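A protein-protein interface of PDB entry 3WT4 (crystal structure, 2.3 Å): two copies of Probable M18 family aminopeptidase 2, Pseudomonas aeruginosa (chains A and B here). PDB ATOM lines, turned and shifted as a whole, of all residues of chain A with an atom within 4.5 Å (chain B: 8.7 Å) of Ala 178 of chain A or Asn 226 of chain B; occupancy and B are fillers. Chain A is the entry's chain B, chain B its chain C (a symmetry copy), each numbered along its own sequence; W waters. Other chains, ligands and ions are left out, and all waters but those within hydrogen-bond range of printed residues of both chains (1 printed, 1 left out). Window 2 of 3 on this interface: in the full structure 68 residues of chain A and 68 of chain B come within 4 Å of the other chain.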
ATOM      1  N   GLY A 100       7.599 -22.580 -39.940  1.00  0.00           N
ATOM      2  CA  GLY A 100       6.888 -22.483 -38.712  1.00  0.00           C
ATOM      3  C   GLY A 100       7.702 -21.763 -37.643  1.00  0.00           C
ATOM      4  O   GLY A 100       7.186 -21.526 -36.565  1.00  0.00           O
ATOM      5  N   PHE A 101       8.938 -21.346 -37.932  1.00  0.00           N
ATOM      6  CA  PHE A 101       9.723 -20.556 -36.950  1.00  0.00           C
ATOM      7  C   PHE A 101       9.677 -19.038 -37.196  1.00  0.00           C
ATOM      8  O   PHE A 101       9.529 -18.568 -38.319  1.00  0.00           O
ATOM      9  CB  PHE A 101      11.184 -20.955 -36.948  1.00  0.00           C
ATOM     10  CG  PHE A 101      11.418 -22.384 -36.643  1.00  0.00           C
ATOM     11  CD1 PHE A 101      11.398 -22.830 -35.319  1.00  0.00           C
ATOM     12  CD2 PHE A 101      11.553 -23.308 -37.672  1.00  0.00           C
ATOM     13  CE1 PHE A 101      11.644 -24.133 -35.044  1.00  0.00           C
ATOM     14  CE2 PHE A 101      11.752 -24.641 -37.402  1.00  0.00           C
ATOM     15  CZ  PHE A 101      11.811 -25.053 -36.092  1.00  0.00           C
ATOM     16  N   LEU A 102       9.928 -18.304 -36.142  1.00  0.00           N
ATOM     17  CA  LEU A 102      10.343 -16.922 -36.231  1.00  0.00           C
ATOM     18  C   LEU A 102      11.841 -16.865 -35.904  1.00  0.00           C
ATOM     19  O   LEU A 102      12.301 -17.302 -34.828  1.00  0.00           O
ATOM     20  CB  LEU A 102       9.566 -16.053 -35.225  1.00  0.00           C
ATOM     21  CG  LEU A 102       9.985 -14.602 -35.149  1.00  0.00           C
ATOM     22  CD1 LEU A 102       9.808 -13.905 -36.468  1.00  0.00           C
ATOM     23  CD2 LEU A 102       9.181 -13.857 -34.127  1.00  0.00           C
ATOM     24  N   ILE A 176      16.959 -18.673 -34.352  1.00  0.00           N
ATOM     25  CA  ILE A 176      15.563 -19.016 -33.994  1.00  0.00           C
ATOM     26  C   ILE A 176      15.275 -18.522 -32.599  1.00  0.00           C
ATOM     27  O   ILE A 176      16.034 -18.760 -31.667  1.00  0.00           O
ATOM     28  CB  ILE A 176      15.340 -20.554 -34.013  1.00  0.00           C
ATOM     29  CG1 ILE A 176      15.716 -21.102 -35.389  1.00  0.00           C
ATOM     30  CG2 ILE A 176      13.883 -20.936 -33.754  1.00  0.00           C
ATOM     31  CD1 ILE A 176      15.706 -22.618 -35.451  1.00  0.00           C
ATOM     32  N   ILE A 177      14.189 -17.784 -32.490  1.00  0.00           N
ATOM     33  CA  ILE A 177      13.651 -17.265 -31.215  1.00  0.00           C
ATOM     34  C   ILE A 177      12.251 -17.817 -30.861  1.00  0.00           C
ATOM     35  O   ILE A 177      11.868 -17.845 -29.686  1.00  0.00           O
ATOM     36  CB  ILE A 177      13.586 -15.725 -31.158  1.00  0.00           C
ATOM     37  CG1 ILE A 177      12.453 -15.183 -32.024  1.00  0.00           C
ATOM     38  CG2 ILE A 177      14.904 -15.039 -31.556  1.00  0.00           C
ATOM     39  CD1 ILE A 177      12.222 -13.709 -31.733  1.00  0.00           C
ATOM     40  N   ALA A 178      11.498 -18.293 -31.842  1.00  0.00           N
ATOM     41  CA  ALA A 178      10.188 -18.798 -31.539  1.00  0.00           C
ATOM     42  C   ALA A 178       9.576 -19.660 -32.674  1.00  0.00           C
ATOM     43  O   ALA A 178      10.130 -19.801 -33.745  1.00  0.00           O
ATOM     44  CB  ALA A 178       9.246 -17.632 -31.183  1.00  0.00           C
ATOM     45  N   GLN A 179       8.414 -20.228 -32.378  1.00  0.00           N
ATOM     46  CA  GLN A 179       7.559 -20.830 -33.372  1.00  0.00           C
ATOM     47  C   GLN A 179       6.304 -19.965 -33.477  1.00  0.00           C
ATOM     48  O   GLN A 179       5.898 -19.338 -32.523  1.00  0.00           O
ATOM     49  CB  GLN A 179       7.242 -22.241 -32.932  1.00  0.00           C
ATOM     50  CG  GLN A 179       8.392 -23.159 -33.220  1.00  0.00           C
ATOM     51  CD  GLN A 179       8.159 -24.545 -32.751  1.00  0.00           C
ATOM     52  OE1 GLN A 179       7.827 -24.771 -31.607  1.00  0.00           O
ATOM     53  NE2 GLN A 179       8.345 -25.501 -33.635  1.00  0.00           N
ATOM     54  N   LEU A 180       5.742 -19.894 -34.654  1.00  0.00           N
ATOM     55  CA  LEU A 180       4.545 -19.090 -34.922  1.00  0.00           C
ATOM     56  C   LEU A 180       3.333 -19.964 -35.189  1.00  0.00           C
ATOM     57  O   LEU A 180       3.410 -20.929 -35.945  1.00  0.00           O
ATOM     58  CB  LEU A 180       4.771 -18.259 -36.186  1.00  0.00           C
ATOM     59  CG  LEU A 180       5.851 -17.193 -36.089  1.00  0.00           C
ATOM     60  CD1 LEU A 180       6.272 -16.693 -37.450  1.00  0.00           C
ATOM     61  CD2 LEU A 180       5.337 -16.061 -35.230  1.00  0.00           C
ATOM     62  N   ARG B   2       4.172 -31.275 -18.452  1.00  0.00           N
ATOM     63  CA  ARG B   2       5.296 -31.183 -19.306  1.00  0.00           C
ATOM     64  C   ARG B   2       6.544 -30.593 -18.592  1.00  0.00           C
ATOM     65  O   ARG B   2       7.666 -31.095 -18.731  1.00  0.00           O
ATOM     66  CB  ARG B   2       4.895 -30.355 -20.521  1.00  0.00           C
ATOM     67  CG  ARG B   2       5.964 -29.381 -20.970  1.00  0.00           C
ATOM     68  CD  ARG B   2       5.411 -28.294 -21.879  1.00  0.00           C
ATOM     69  NE  ARG B   2       4.436 -28.895 -22.778  1.00  0.00           N
ATOM     70  CZ  ARG B   2       3.180 -28.494 -22.917  1.00  0.00           C
ATOM     71  NH1 ARG B   2       2.717 -27.431 -22.243  1.00  0.00           N
ATOM     72  NH2 ARG B   2       2.398 -29.150 -23.772  1.00  0.00           N
ATOM     73  N   VAL B 222      15.712 -25.093 -20.865  1.00  0.00           N
ATOM     74  CA  VAL B 222      14.636 -24.686 -21.742  1.00  0.00           C
ATOM     75  C   VAL B 222      15.113 -23.391 -22.392  1.00  0.00           C
ATOM     76  O   VAL B 222      15.855 -22.669 -21.794  1.00  0.00           O
ATOM     77  CB  VAL B 222      13.383 -24.523 -20.920  1.00  0.00           C
ATOM     78  CG1 VAL B 222      12.195 -24.137 -21.768  1.00  0.00           C
ATOM     79  CG2 VAL B 222      13.119 -25.835 -20.210  1.00  0.00           C
ATOM     80  N   VAL B 223      14.838 -23.189 -23.666  1.00  0.00           N
ATOM     81  CA  VAL B 223      15.298 -22.013 -24.398  1.00  0.00           C
ATOM     82  C   VAL B 223      14.171 -21.579 -25.342  1.00  0.00           C
ATOM     83  O   VAL B 223      13.290 -22.395 -25.759  1.00  0.00           O
ATOM     84  CB  VAL B 223      16.605 -22.253 -25.202  1.00  0.00           C
ATOM     85  CG1 VAL B 223      17.726 -22.764 -24.352  1.00  0.00           C
ATOM     86  CG2 VAL B 223      16.418 -23.233 -26.282  1.00  0.00           C
ATOM     87  N   GLY B 224      14.150 -20.297 -25.674  1.00  0.00           N
ATOM     88  CA  GLY B 224      13.158 -19.803 -26.567  1.00  0.00           C
ATOM     89  C   GLY B 224      12.248 -18.752 -25.958  1.00  0.00           C
ATOM     90  O   GLY B 224      11.973 -18.750 -24.772  1.00  0.00           O
ATOM     91  N   LEU B 225      11.787 -17.849 -26.815  1.00  0.00           N
ATOM     92  CA  LEU B 225      10.925 -16.787 -26.397  1.00  0.00           C
ATOM     93  C   LEU B 225       9.728 -17.322 -25.608  1.00  0.00           C
ATOM     94  O   LEU B 225       9.346 -16.759 -24.625  1.00  0.00           O
ATOM     95  CB  LEU B 225      10.446 -16.018 -27.615  1.00  0.00           C
ATOM     96  CG  LEU B 225       9.603 -14.809 -27.207  1.00  0.00           C
ATOM     97  CD1 LEU B 225      10.448 -13.826 -26.392  1.00  0.00           C
ATOM     98  CD2 LEU B 225       8.986 -14.154 -28.434  1.00  0.00           C
ATOM     99  N   ASN B 226       9.138 -18.397 -26.067  1.00  0.00           N
ATOM    100  CA  ASN B 226       8.020 -19.005 -25.373  1.00  0.00           C
ATOM    101  C   ASN B 226       8.371 -20.408 -24.847  1.00  0.00           C
ATOM    102  O   ASN B 226       7.484 -21.247 -24.757  1.00  0.00           O
ATOM    103  CB  ASN B 226       6.808 -19.094 -26.287  1.00  0.00           C
ATOM    104  CG  ASN B 226       6.532 -17.778 -26.982  1.00  0.00           C
ATOM    105  OD1 ASN B 226       6.138 -16.826 -26.345  1.00  0.00           O
ATOM    106  ND2 ASN B 226       6.800 -17.702 -28.266  1.00  0.00           N
ATOM    107  N   ASP B 227       9.652 -20.631 -24.501  1.00  0.00           N
ATOM    108  CA  ASP B 227      10.102 -21.918 -23.953  1.00  0.00           C
ATOM    109  C   ASP B 227       9.779 -23.072 -24.858  1.00  0.00           C
ATOM    110  O   ASP B 227       9.359 -24.162 -24.400  1.00  0.00           O
ATOM    111  CB  ASP B 227       9.472 -22.145 -22.564  1.00  0.00           C
ATOM    112  CG  ASP B 227       9.857 -21.065 -21.556  1.00  0.00           C
ATOM    113  OD1 ASP B 227      10.860 -20.310 -21.675  1.00  0.00           O
ATOM    114  OD2 ASP B 227       9.114 -20.943 -20.617  1.00  0.00           O
ATOM    115  N   GLU B 228       9.955 -22.845 -26.157  1.00  0.00           N
ATOM    116  CA  GLU B 228       9.613 -23.843 -27.137  1.00  0.00           C
ATOM    117  C   GLU B 228      10.549 -25.030 -27.182  1.00  0.00           C
ATOM    118  O   GLU B 228      10.205 -26.086 -27.718  1.00  0.00           O
ATOM    119  CB  GLU B 228       9.611 -23.190 -28.516  1.00  0.00           C
ATOM    120  CG  GLU B 228       8.442 -22.255 -28.755  1.00  0.00           C
ATOM    121  CD  GLU B 228       8.846 -20.806 -28.631  1.00  0.00           C
ATOM    122  OE1 GLU B 228       9.845 -20.404 -27.879  1.00  0.00           O
ATOM    123  OE2 GLU B 228       8.112 -20.078 -29.314  1.00  0.00           O
ATOM    124  N   PHE B 229      11.764 -24.813 -26.727  1.00  0.00           N
ATOM    125  CA  PHE B 229      12.842 -25.726 -26.982  1.00  0.00           C
ATOM    126  C   PHE B 229      13.589 -26.216 -25.752  1.00  0.00           C
ATOM    127  O   PHE B 229      13.606 -25.569 -24.675  1.00  0.00           O
ATOM    128  CB  PHE B 229      13.859 -25.064 -27.905  1.00  0.00           C
ATOM    129  CG  PHE B 229      13.259 -24.340 -29.102  1.00  0.00           C
ATOM    130  CD1 PHE B 229      12.593 -25.020 -30.073  1.00  0.00           C
ATOM    131  CD2 PHE B 229      13.406 -22.950 -29.243  1.00  0.00           C
ATOM    132  CE1 PHE B 229      12.016 -24.361 -31.158  1.00  0.00           C
ATOM    133  CE2 PHE B 229      12.870 -22.281 -30.369  1.00  0.00           C
ATOM    134  CZ  PHE B 229      12.156 -22.993 -31.323  1.00  0.00           C
ATOM    135  N   PRO B 314      15.374 -24.330 -40.543  1.00  0.00           N
ATOM    136  CA  PRO B 314      15.056 -23.252 -41.469  1.00  0.00           C
ATOM    137  C   PRO B 314      16.239 -22.567 -42.101  1.00  0.00           C
ATOM    138  O   PRO B 314      16.041 -21.841 -43.041  1.00  0.00           O
ATOM    139  CB  PRO B 314      14.302 -22.240 -40.585  1.00  0.00           C
ATOM    140  CG  PRO B 314      14.835 -22.505 -39.179  1.00  0.00           C
ATOM    141  CD  PRO B 314      15.059 -23.998 -39.137  1.00  0.00           C
ATOM    142  N   ASN B 329       8.106 -29.919 -31.795  1.00  0.00           N
ATOM    143  CA  ASN B 329       6.821 -29.732 -31.110  1.00  0.00           C
ATOM    144  C   ASN B 329       5.626 -30.169 -31.911  1.00  0.00           C
ATOM    145  O   ASN B 329       4.492 -29.880 -31.556  1.00  0.00           O
ATOM    146  CB  ASN B 329       6.658 -28.299 -30.592  1.00  0.00           C
ATOM    147  CG  ASN B 329       7.640 -27.985 -29.514  1.00  0.00           C
ATOM    148  OD1 ASN B 329       7.841 -28.799 -28.594  1.00  0.00           O
ATOM    149  ND2 ASN B 329       8.328 -26.848 -29.644  1.00  0.00           N
ATOM    150  N   PHE B 398      17.383 -30.766 -33.766  1.00  0.00           N
ATOM    151  CA  PHE B 398      18.412 -30.170 -34.616  1.00  0.00           C
ATOM    152  C   PHE B 398      19.813 -30.453 -34.053  1.00  0.00           C
ATOM    153  O   PHE B 398      19.957 -30.677 -32.863  1.00  0.00           O
ATOM    154  CB  PHE B 398      18.278 -28.648 -34.626  1.00  0.00           C
ATOM    155  CG  PHE B 398      17.053 -28.116 -35.282  1.00  0.00           C
ATOM    156  CD1 PHE B 398      16.502 -28.729 -36.396  1.00  0.00           C
ATOM    157  CD2 PHE B 398      16.490 -26.942 -34.803  1.00  0.00           C
ATOM    158  CE1 PHE B 398      15.359 -28.197 -36.981  1.00  0.00           C
ATOM    159  CE2 PHE B 398      15.353 -26.393 -35.374  1.00  0.00           C
ATOM    160  CZ  PHE B 398      14.770 -27.017 -36.469  1.00  0.00           C
ATOM    161  N   SER B 409      10.324 -28.625 -26.545  1.00  0.00           N
ATOM    162  CA  SER B 409       9.938 -28.801 -25.150  1.00  0.00           C
ATOM    163  C   SER B 409       8.558 -29.454 -24.973  1.00  0.00           C
ATOM    164  O   SER B 409       8.203 -29.761 -23.872  1.00  0.00           O
ATOM    165  CB  SER B 409       9.949 -27.442 -24.435  1.00  0.00           C
ATOM    166  OG  SER B 409       8.936 -26.617 -24.985  1.00  0.00           O
ATOM    167  N   HIS B 410       7.760 -29.613 -26.024  1.00  0.00           N
ATOM    168  CA  HIS B 410       6.451 -30.250 -25.916  1.00  0.00           C
ATOM    169  C   HIS B 410       6.548 -31.731 -26.263  1.00  0.00           C
ATOM    170  O   HIS B 410       5.624 -32.482 -26.034  1.00  0.00           O
ATOM    171  CB  HIS B 410       5.470 -29.611 -26.910  1.00  0.00           C
ATOM    172  CG  HIS B 410       5.121 -28.192 -26.576  1.00  0.00           C
ATOM    173  ND1 HIS B 410       3.846 -27.695 -26.667  1.00  0.00           N
ATOM    174  CD2 HIS B 410       5.867 -27.185 -26.079  1.00  0.00           C
ATOM    175  CE1 HIS B 410       3.819 -26.453 -26.235  1.00  0.00           C
ATOM    176  NE2 HIS B 410       5.038 -26.115 -25.888  1.00  0.00           N
HETATM  177  O   HOH W   1       5.779 -20.713 -29.775  1.00  0.00           O
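Of the printed residues of chain B, Ile 177 of chain A touches Gly 224 (3.9 Å), Leu 225 (2.9 Å) and Glu 228 (3.7 Å).
Ala 178 of chain A touches just these residues of chain B: Asn 226 (3.8 Å) and Glu 228 (3.3 Å).
Of the printed residues of chain B, Gln 179 of chain A touches Glu 228 (3.1 Å) and Asn 329 (2.9 Å).
Of the printed residues of chain A, Leu 225 of chain B touches Ile 177.
Asn 226 of chain B touches just one residue of chain A: Ala 178.
Printed residues of chain A within 4 Å of Phe 229 of chain B: Phe 101 (3.9 Å) and Ile 176 (3.6 Å).
Of the printed residues of chain A, Phe 398 of chain B touches Phe 101 and Ile 176.
The nearest residue of chain B that does not touch Ala 178 of chain A is Leu 225 of chain B (4.1 Å).
The nearest printed residue of chain A that does not touch Phe 398 of chain B is Gln 179 of chain A (7.2 Å).
The backbone NH (N) of Leu 225 of chain B is in hydrogen-bond range of the backbone carbonyl oxygen (O) of Ile 177 of chain A (2.9 Å).
The side-chain carboxylate (OE2) of Glu 228 of chain B is in hydrogen-bond range of the backbone NH (N) of Gln 179 of chain A, at 3.1 Å.
The side-chain amide nitrogen (ND2) of Asn 329 of chain B lies within hydrogen-bond range of the side-chain amide oxygen (OE1) of Gln 179 of chain A.
Water W1 lies within hydrogen-bond range of OE2 of Glu 228 of chain B (2.5 Å) and O of Gln 179 of chain A (3.1 Å).
The backbone NH (N) of Ile 177 of chain A sits at hydrogen-bond distance from the backbone carbonyl oxygen (O) of Leu 102 of chain A (3.0 Å).
The backbone NH of Leu 102 of chain A is in hydrogen-bond range of the backbone carbonyl oxygen of Ala 178 of chain A (2.8 Å).
The backbone NH (N) of Glu 228 of chain B is in hydrogen-bond range of the backbone carbonyl oxygen (O) of Val 223 of chain B.
N of Leu 225 of chain B sits at hydrogen-bond distance from OE1 of Glu 228 of chain B.
The backbone carbonyl oxygen (O) of Glu 228 of chain B sits at hydrogen-bond distance from the side-chain amide nitrogen (ND2) of Asn 329 of chain B.
N of Ser 409 of chain B sits at hydrogen-bond distance from O of Glu 228 of chain B, 2.8 Å away.
No position is printed for both chains.
Of the 13 pairs that touch across the chains among the printed residues, none has its exchanged pair printed and touching as well.
Of the 8 printed residues of chain A, 5 touch a printed residue of chain B.
Printed residues of chain A that touch a printed residue of chain B: Phe 101, Ile 176, Ile 177, Ala 178 and Gln 179.
Hydrophobic or aromatic side chains of chain A within 4 Å of the printed part of chain B: Phe 101, Ile 176 and Ala 178.
Along chain A the printed residues that touch a printed residue of chain B span positions 101 to 179.
Printed residues of chain B that touch a printed residue of chain A: Gly 224, Leu 225, Asn 226, Glu 228, Phe 229, Pro 314, Asn 329 and Phe 398.
Hydrophobic or aromatic side chains of chain B within 4 Å of the printed part of chain A: Leu 225, Phe 229, Pro 314 and Phe 398.
Among the printed residues, pairs that only touch across the chains: Ala 178 of chain A with Glu 228 of chain B, Phe 101 of chain A with Phe 398 of chain B, Ile 176 of chain A with Phe 229 of chain B, Phe 101 of chain A with Pro 314 of chain B, Ile 177 of chain A with Glu 228 of chain B, Ile 176 of chain A with Phe 398 of chain B, Ala 178 of chain A with Asn 226 of chain B, Ile 176 of chain A with Pro 314 of chain B, Ile 177 of chain A with Gly 224 of chain B and Phe 101 of chain A with Phe 229 of chain B.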
